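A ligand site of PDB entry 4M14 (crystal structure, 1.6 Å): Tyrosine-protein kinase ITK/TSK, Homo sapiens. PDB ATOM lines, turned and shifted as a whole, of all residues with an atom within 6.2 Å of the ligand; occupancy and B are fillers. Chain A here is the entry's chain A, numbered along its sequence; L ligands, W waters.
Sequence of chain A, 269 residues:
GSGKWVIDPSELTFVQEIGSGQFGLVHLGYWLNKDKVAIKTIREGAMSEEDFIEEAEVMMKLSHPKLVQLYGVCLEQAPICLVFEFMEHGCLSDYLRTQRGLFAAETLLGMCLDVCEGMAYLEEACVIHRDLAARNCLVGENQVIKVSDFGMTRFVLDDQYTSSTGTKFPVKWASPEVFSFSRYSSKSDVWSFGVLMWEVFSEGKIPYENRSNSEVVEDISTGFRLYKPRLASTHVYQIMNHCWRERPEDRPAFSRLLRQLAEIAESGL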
ATOM      1  N   ILE A  18       8.766 -18.721  27.806  1.00  0.00           N
ATOM      2  CA  ILE A  18       8.809 -17.935  26.580  1.00  0.00           C
ATOM      3  C   ILE A  18       7.382 -17.406  26.342  1.00  0.00           C
ATOM      4  O   ILE A  18       7.201 -16.218  26.116  1.00  0.00           O
ATOM      5  CB  ILE A  18       9.360 -18.857  25.448  1.00  0.00           C
ATOM      6  CG1 ILE A  18      10.896 -18.755  25.328  1.00  0.00           C
ATOM      7  CG2 ILE A  18       8.709 -18.611  24.128  1.00  0.00           C
ATOM      8  CD1 ILE A  18      11.531 -19.779  24.304  1.00  0.00           C
ATOM      9  N   GLY A  19       6.391 -18.283  26.469  1.00  0.00           N
ATOM     10  CA  GLY A  19       4.988 -17.899  26.307  1.00  0.00           C
ATOM     11  C   GLY A  19       4.034 -19.065  26.343  1.00  0.00           C
ATOM     12  O   GLY A  19       4.431 -20.194  26.618  1.00  0.00           O
ATOM     13  N   SER A  20       2.750 -18.776  26.062  1.00  0.00           N
ATOM     14  CA  SER A  20       1.708 -19.785  26.035  1.00  0.00           C
ATOM     15  C   SER A  20       1.311 -20.012  24.588  1.00  0.00           C
ATOM     16  O   SER A  20       0.798 -19.100  23.931  1.00  0.00           O
ATOM     17  CB  SER A  20       0.502 -19.318  26.853  1.00  0.00           C
ATOM     18  OG  SER A  20       0.849 -18.960  28.184  1.00  0.00           O
ATOM     19  N   GLY A  21       1.586 -21.206  24.077  1.00  0.00           N
ATOM     20  CA  GLY A  21       1.259 -21.606  22.711  1.00  0.00           C
ATOM     21  C   GLY A  21      -0.144 -22.169  22.578  1.00  0.00           C
ATOM     22  O   GLY A  21      -0.964 -22.027  23.503  1.00  0.00           O
ATOM     23  N   VAL A  26       5.532 -22.845  26.362  1.00  0.00           N
ATOM     24  CA  VAL A  26       6.785 -22.929  25.620  1.00  0.00           C
ATOM     25  C   VAL A  26       7.837 -22.341  26.552  1.00  0.00           C
ATOM     26  O   VAL A  26       7.637 -21.246  27.100  1.00  0.00           O
ATOM     27  CB  VAL A  26       6.780 -22.188  24.254  1.00  0.00           C
ATOM     28  CG1 VAL A  26       8.113 -22.391  23.517  1.00  0.00           C
ATOM     29  CG2 VAL A  26       5.606 -22.637  23.376  1.00  0.00           C
ATOM     30  N   VAL A  37      17.567 -25.034  24.000  1.00  0.00           N
ATOM     31  CA  VAL A  37      16.414 -25.511  23.269  1.00  0.00           C
ATOM     32  C   VAL A  37      15.133 -24.756  23.603  1.00  0.00           C
ATOM     33  O   VAL A  37      15.041 -24.105  24.660  1.00  0.00           O
ATOM     34  CB  VAL A  37      16.198 -27.042  23.559  1.00  0.00           C
ATOM     35  CG1 VAL A  37      17.271 -27.915  22.893  1.00  0.00           C
ATOM     36  CG2 VAL A  37      16.072 -27.344  25.059  1.00  0.00           C
ATOM     37  N   ALA A  38      14.123 -24.898  22.715  1.00  0.00           N
ATOM     38  CA  ALA A  38      12.762 -24.438  22.985  1.00  0.00           C
ATOM     39  C   ALA A  38      11.992 -25.718  23.319  1.00  0.00           C
ATOM     40  O   ALA A  38      12.110 -26.728  22.617  1.00  0.00           O
ATOM     41  CB  ALA A  38      12.156 -23.774  21.755  1.00  0.00           C
ATOM     42  N   LYS A  40       8.293 -27.372  24.101  1.00  0.00           N
ATOM     43  CA  LYS A  40       6.857 -27.149  23.995  1.00  0.00           C
ATOM     44  C   LYS A  40       6.143 -28.253  24.765  1.00  0.00           C
ATOM     45  O   LYS A  40       6.287 -29.421  24.432  1.00  0.00           O
ATOM     46  CB  LYS A  40       6.382 -27.104  22.535  1.00  0.00           C
ATOM     47  CG  LYS A  40       7.027 -25.984  21.728  1.00  0.00           C
ATOM     48  CD  LYS A  40       6.264 -25.740  20.445  1.00  0.00           C
ATOM     49  CE  LYS A  40       6.724 -24.479  19.783  1.00  0.00           C
ATOM     50  NZ  LYS A  40       5.844 -24.103  18.640  1.00  0.00           N
ATOM     51  N   VAL A  68      13.599 -26.113  11.099  1.00  0.00           N
ATOM     52  CA  VAL A  68      13.784 -26.130  12.564  1.00  0.00           C
ATOM     53  C   VAL A  68      13.917 -27.612  12.995  1.00  0.00           C
ATOM     54  O   VAL A  68      13.008 -28.413  12.751  1.00  0.00           O
ATOM     55  CB  VAL A  68      12.614 -25.419  13.305  1.00  0.00           C
ATOM     56  CG1 VAL A  68      12.776 -25.538  14.823  1.00  0.00           C
ATOM     57  CG2 VAL A  68      12.484 -23.939  12.910  1.00  0.00           C
ATOM     58  N   PHE A  84      12.859 -28.595  20.668  1.00  0.00           N
ATOM     59  CA  PHE A  84      13.289 -28.050  19.391  1.00  0.00           C
ATOM     60  C   PHE A  84      14.545 -27.206  19.515  1.00  0.00           C
ATOM     61  O   PHE A  84      14.867 -26.665  20.568  1.00  0.00           O
ATOM     62  CB  PHE A  84      12.199 -27.080  18.865  1.00  0.00           C
ATOM     63  CG  PHE A  84      10.854 -27.687  18.548  1.00  0.00           C
ATOM     64  CD1 PHE A  84      10.541 -28.072  17.243  1.00  0.00           C
ATOM     65  CD2 PHE A  84       9.865 -27.785  19.523  1.00  0.00           C
ATOM     66  CE1 PHE A  84       9.272 -28.596  16.943  1.00  0.00           C
ATOM     67  CE2 PHE A  84       8.609 -28.338  19.226  1.00  0.00           C
ATOM     68  CZ  PHE A  84       8.306 -28.704  17.932  1.00  0.00           C
ATOM     69  N   GLU A  85      15.187 -26.970  18.353  1.00  0.00           N
ATOM     70  CA  GLU A  85      16.248 -26.007  18.172  1.00  0.00           C
ATOM     71  C   GLU A  85      15.619 -24.628  18.583  1.00  0.00           C
ATOM     72  O   GLU A  85      14.461 -24.345  18.221  1.00  0.00           O
ATOM     73  CB  GLU A  85      16.577 -26.044  16.666  1.00  0.00           C
ATOM     74  CG  GLU A  85      17.410 -24.930  16.127  1.00  0.00           C
ATOM     75  CD  GLU A  85      17.658 -25.020  14.643  1.00  0.00           C
ATOM     76  OE1 GLU A  85      17.177 -25.962  13.958  1.00  0.00           O
ATOM     77  OE2 GLU A  85      18.402 -24.136  14.174  1.00  0.00           O
ATOM     78  N   PHE A  86      16.371 -23.791  19.342  1.00  0.00           N
ATOM     79  CA  PHE A  86      15.831 -22.497  19.763  1.00  0.00           C
ATOM     80  C   PHE A  86      16.016 -21.464  18.652  1.00  0.00           C
ATOM     81  O   PHE A  86      17.129 -21.317  18.116  1.00  0.00           O
ATOM     82  CB  PHE A  86      16.500 -22.002  21.069  1.00  0.00           C
ATOM     83  CG  PHE A  86      16.078 -20.616  21.491  1.00  0.00           C
ATOM     84  CD1 PHE A  86      14.744 -20.344  21.802  1.00  0.00           C
ATOM     85  CD2 PHE A  86      17.011 -19.603  21.615  1.00  0.00           C
ATOM     86  CE1 PHE A  86      14.362 -19.054  22.209  1.00  0.00           C
ATOM     87  CE2 PHE A  86      16.627 -18.329  22.041  1.00  0.00           C
ATOM     88  CZ  PHE A  86      15.312 -18.067  22.343  1.00  0.00           C
ATOM     89  N   MET A  87      14.925 -20.777  18.322  1.00  0.00           N
ATOM     90  CA  MET A  87      14.855 -19.781  17.242  1.00  0.00           C
ATOM     91  C   MET A  87      14.639 -18.440  17.947  1.00  0.00           C
ATOM     92  O   MET A  87      13.525 -18.095  18.324  1.00  0.00           O
ATOM     93  CB  MET A  87      13.723 -20.134  16.275  1.00  0.00           C
ATOM     94  CG  MET A  87      13.928 -21.484  15.568  1.00  0.00           C
ATOM     95  SD  MET A  87      15.432 -21.557  14.582  1.00  0.00           S
ATOM     96  CE  MET A  87      14.942 -20.452  13.198  1.00  0.00           C
ATOM     97  N   GLU A  88      15.718 -17.697  18.088  1.00  0.00           N
ATOM     98  CA  GLU A  88      15.772 -16.466  18.895  1.00  0.00           C
ATOM     99  C   GLU A  88      14.775 -15.369  18.612  1.00  0.00           C
ATOM    100  O   GLU A  88      14.364 -14.652  19.529  1.00  0.00           O
ATOM    101  CB  GLU A  88      17.216 -15.923  19.034  1.00  0.00           C
ATOM    102  CG  GLU A  88      17.829 -15.353  17.777  1.00  0.00           C
ATOM    103  CD  GLU A  88      19.216 -14.776  17.991  1.00  0.00           C
ATOM    104  OE1 GLU A  88      19.324 -13.725  18.655  1.00  0.00           O
ATOM    105  OE2 GLU A  88      20.190 -15.379  17.490  1.00  0.00           O
ATOM    106  N   HIS A  89      14.385 -15.218  17.332  1.00  0.00           N
ATOM    107  CA  HIS A  89      13.443 -14.133  16.993  1.00  0.00           C
ATOM    108  C   HIS A  89      11.982 -14.524  16.858  1.00  0.00           C
ATOM    109  O   HIS A  89      11.168 -13.688  16.452  1.00  0.00           O
ATOM    110  CB  HIS A  89      13.946 -13.314  15.803  1.00  0.00           C
ATOM    111  CG  HIS A  89      15.207 -12.579  16.103  1.00  0.00           C
ATOM    112  ND1 HIS A  89      16.409 -12.969  15.535  1.00  0.00           N
ATOM    113  CD2 HIS A  89      15.428 -11.540  16.935  1.00  0.00           C
ATOM    114  CE1 HIS A  89      17.315 -12.127  16.015  1.00  0.00           C
ATOM    115  NE2 HIS A  89      16.782 -11.269  16.871  1.00  0.00           N
ATOM    116  N   GLY A  90      11.645 -15.772  17.183  1.00  0.00           N
ATOM    117  CA  GLY A  90      10.266 -16.219  17.179  1.00  0.00           C
ATOM    118  C   GLY A  90       9.618 -16.398  15.829  1.00  0.00           C
ATOM    119  O   GLY A  90      10.311 -16.591  14.831  1.00  0.00           O
ATOM    120  N   CYS A  91       8.266 -16.388  15.798  1.00  0.00           N
ATOM    121  CA  CYS A  91       7.581 -16.647  14.540  1.00  0.00           C
ATOM    122  C   CYS A  91       7.694 -15.531  13.533  1.00  0.00           C
ATOM    123  O   CYS A  91       7.712 -14.342  13.878  1.00  0.00           O
ATOM    124  CB  CYS A  91       6.151 -17.135  14.734  1.00  0.00           C
ATOM    125  SG  CYS A  91       5.001 -15.824  15.200  1.00  0.00           S
ATOM    126  N   ASP A  94       4.864 -12.648  13.433  1.00  0.00           N
ATOM    127  CA  ASP A  94       5.040 -11.562  14.415  1.00  0.00           C
ATOM    128  C   ASP A  94       6.262 -10.698  14.103  1.00  0.00           C
ATOM    129  O   ASP A  94       6.230  -9.487  14.285  1.00  0.00           O
ATOM    130  CB  ASP A  94       5.170 -12.138  15.838  1.00  0.00           C
ATOM    131  CG  ASP A  94       3.882 -12.751  16.363  1.00  0.00           C
ATOM    132  OD1 ASP A  94       2.811 -12.393  15.854  1.00  0.00           O
ATOM    133  OD2 ASP A  94       3.967 -13.586  17.285  1.00  0.00           O
ATOM    134  N   ARG A 135       3.130 -18.029  10.221  1.00  0.00           N
ATOM    135  CA  ARG A 135       3.002 -18.361  11.659  1.00  0.00           C
ATOM    136  C   ARG A 135       3.768 -19.627  12.044  1.00  0.00           C
ATOM    137  O   ARG A 135       4.100 -19.771  13.221  1.00  0.00           O
ATOM    138  CB  ARG A 135       1.518 -18.464  12.083  1.00  0.00           C
ATOM    139  CG  ARG A 135       0.723 -19.507  11.279  1.00  0.00           C
ATOM    140  CD  ARG A 135      -0.790 -19.506  11.533  1.00  0.00           C
ATOM    141  NE  ARG A 135      -1.523 -20.020  10.364  1.00  0.00           N
ATOM    142  CZ  ARG A 135      -1.607 -21.312  10.026  1.00  0.00           C
ATOM    143  NH1 ARG A 135      -1.041 -22.248  10.782  1.00  0.00           N
ATOM    144  NH2 ARG A 135      -2.275 -21.672   8.945  1.00  0.00           N
ATOM    145  N   LEU A 138      10.024 -19.870  11.534  1.00  0.00           N
ATOM    146  CA  LEU A 138      10.710 -19.233  12.650  1.00  0.00           C
ATOM    147  C   LEU A 138      11.949 -18.492  12.210  1.00  0.00           C
ATOM    148  O   LEU A 138      12.533 -18.814  11.170  1.00  0.00           O
ATOM    149  CB  LEU A 138      10.997 -20.272  13.792  1.00  0.00           C
ATOM    150  CG  LEU A 138       9.739 -21.037  14.291  1.00  0.00           C
ATOM    151  CD1 LEU A 138      10.076 -22.133  15.296  1.00  0.00           C
ATOM    152  CD2 LEU A 138       8.740 -20.106  14.950  1.00  0.00           C
ATOM    153  N   SER A 148       8.950 -24.938  10.178  1.00  0.00           N
ATOM    154  CA  SER A 148       8.670 -25.783  11.331  1.00  0.00           C
ATOM    155  C   SER A 148       7.252 -26.337  11.242  1.00  0.00           C
ATOM    156  O   SER A 148       6.441 -25.843  10.461  1.00  0.00           O
ATOM    157  CB  SER A 148       8.792 -24.956  12.596  1.00  0.00           C
ATOM    158  OG  SER A 148       8.747 -25.772  13.759  1.00  0.00           O
ATOM    159  N   ASP A 149       6.943 -27.350  12.063  1.00  0.00           N
ATOM    160  CA  ASP A 149       5.601 -27.927  12.196  1.00  0.00           C
ATOM    161  C   ASP A 149       5.080 -28.691  10.994  1.00  0.00           C
ATOM    162  O   ASP A 149       3.874 -28.908  10.852  1.00  0.00           O
ATOM    163  CB  ASP A 149       4.585 -26.872  12.681  1.00  0.00           C
ATOM    164  CG  ASP A 149       4.852 -26.252  14.054  1.00  0.00           C
ATOM    165  OD1 ASP A 149       5.864 -26.636  14.699  1.00  0.00           O
ATOM    166  OD2 ASP A 149       4.101 -25.334  14.442  1.00  0.00           O
HETATM  167  N1  LIG L   1       9.542 -18.615  20.008  1.00  0.00           N
HETATM  168  N2  LIG L   1       8.388 -18.824  19.353  1.00  0.00           N
HETATM  169  C1  LIG L   1       8.472 -20.085  18.893  1.00  0.00           C
HETATM  170  C2  LIG L   1       9.709 -20.687  19.245  1.00  0.00           C
HETATM  171  C3  LIG L   1      10.373 -19.706  19.946  1.00  0.00           C
HETATM  172  N3  LIG L   1      10.150 -21.971  18.936  1.00  0.00           N
HETATM  173  C4  LIG L   1      11.507 -22.267  18.845  1.00  0.00           C
HETATM  174  N4  LIG L   1      11.710 -23.445  18.175  1.00  0.00           N
HETATM  175  O1  LIG L   1      12.408 -21.551  19.288  1.00  0.00           O
HETATM  176  C5  LIG L   1       7.394 -20.679  18.131  1.00  0.00           C
HETATM  177  N5  LIG L   1       6.394 -19.793  17.804  1.00  0.00           N
HETATM  178  O2  LIG L   1       7.427 -21.855  17.798  1.00  0.00           O
HETATM  179  C6  LIG L   1       9.849 -17.393  20.640  1.00  0.00           C
HETATM  180  C7  LIG L   1      11.149 -16.938  20.505  1.00  0.00           C
HETATM  181  C8  LIG L   1      11.547 -15.767  21.096  1.00  0.00           C
HETATM  182  C9  LIG L   1      10.653 -15.050  21.866  1.00  0.00           C
HETATM  183  C10 LIG L   1       8.932 -16.680  21.401  1.00  0.00           C
HETATM  184  C11 LIG L   1       9.352 -15.507  22.015  1.00  0.00           C
HETATM  185  C12 LIG L   1       8.481 -14.758  22.770  1.00  0.00           C
HETATM  186  C13 LIG L   1       7.183 -15.180  22.954  1.00  0.00           C
HETATM  187  C14 LIG L   1       6.740 -16.332  22.336  1.00  0.00           C
HETATM  188  C15 LIG L   1       7.617 -17.073  21.560  1.00  0.00           C
HETATM  189  O3  LIG L   1       5.422 -16.680  22.618  1.00  0.00           O
HETATM  190  C16 LIG L   1       4.865 -17.685  21.767  1.00  0.00           C
HETATM  191  C17 LIG L   1       4.956 -19.019  22.459  1.00  0.00           C
HETATM  192  C18 LIG L   1       3.405 -17.335  21.618  1.00  0.00           C
HETATM  193  O   HOH W   1       8.830 -14.079  25.961  1.00  0.00           O
HETATM  194  O   HOH W   2       9.246 -24.917  17.261  1.00  0.00           O
HETATM  195  O   HOH W   3       6.936 -16.485  18.201  1.00  0.00           O
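The backbone carbonyl oxygen (O) of Glu 85 sits at hydrogen-bond distance from a nitrogen (N4) of the ligand.
NZ of Lys 40 sits at hydrogen-bond distance from O2 of the ligand, 2.9 Å away.
N of Met 87 lies within hydrogen-bond range of O1 of the ligand (2.8 Å).
The backbone NH (N) of Phe 84 lies within hydrogen-bond range of the backbone carbonyl oxygen (O) of Ala 38 (2.8 Å).
The backbone NH (N) of Val 26 lies within hydrogen-bond range of the backbone carbonyl oxygen (O) of Gly 19, 2.9 Å away.
The backbone NH of Ile 18 lies within hydrogen-bond range of the backbone carbonyl oxygen of Val 26.
Ile 18 touches the ligand.
CA of Gly 19 touches O3 of the ligand, at 3.9 Å.
O of Ser 20 touches C18 of the ligand (3.9 Å).
Val 26 touches the ligand (CG2 to C17, 3.8 Å).
CB of Ala 38 touches O1 of the ligand (3.3 Å).
Phe 84 touches the ligand.
Phe 86 touches the ligand.
Glu 88 touches the ligand.
Gly 90 touches the ligand (CA to C7, 3.5 Å).
CD2 of Leu 138 touches C5 of the ligand, 3.5 Å away.
The nearest printed residue that does not touch the ligand is Cys 91 (4.1 Å).
Water W3 lies within hydrogen-bond range of N of Cys 91 (2.7 Å) and N2 of the ligand (3.0 Å).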
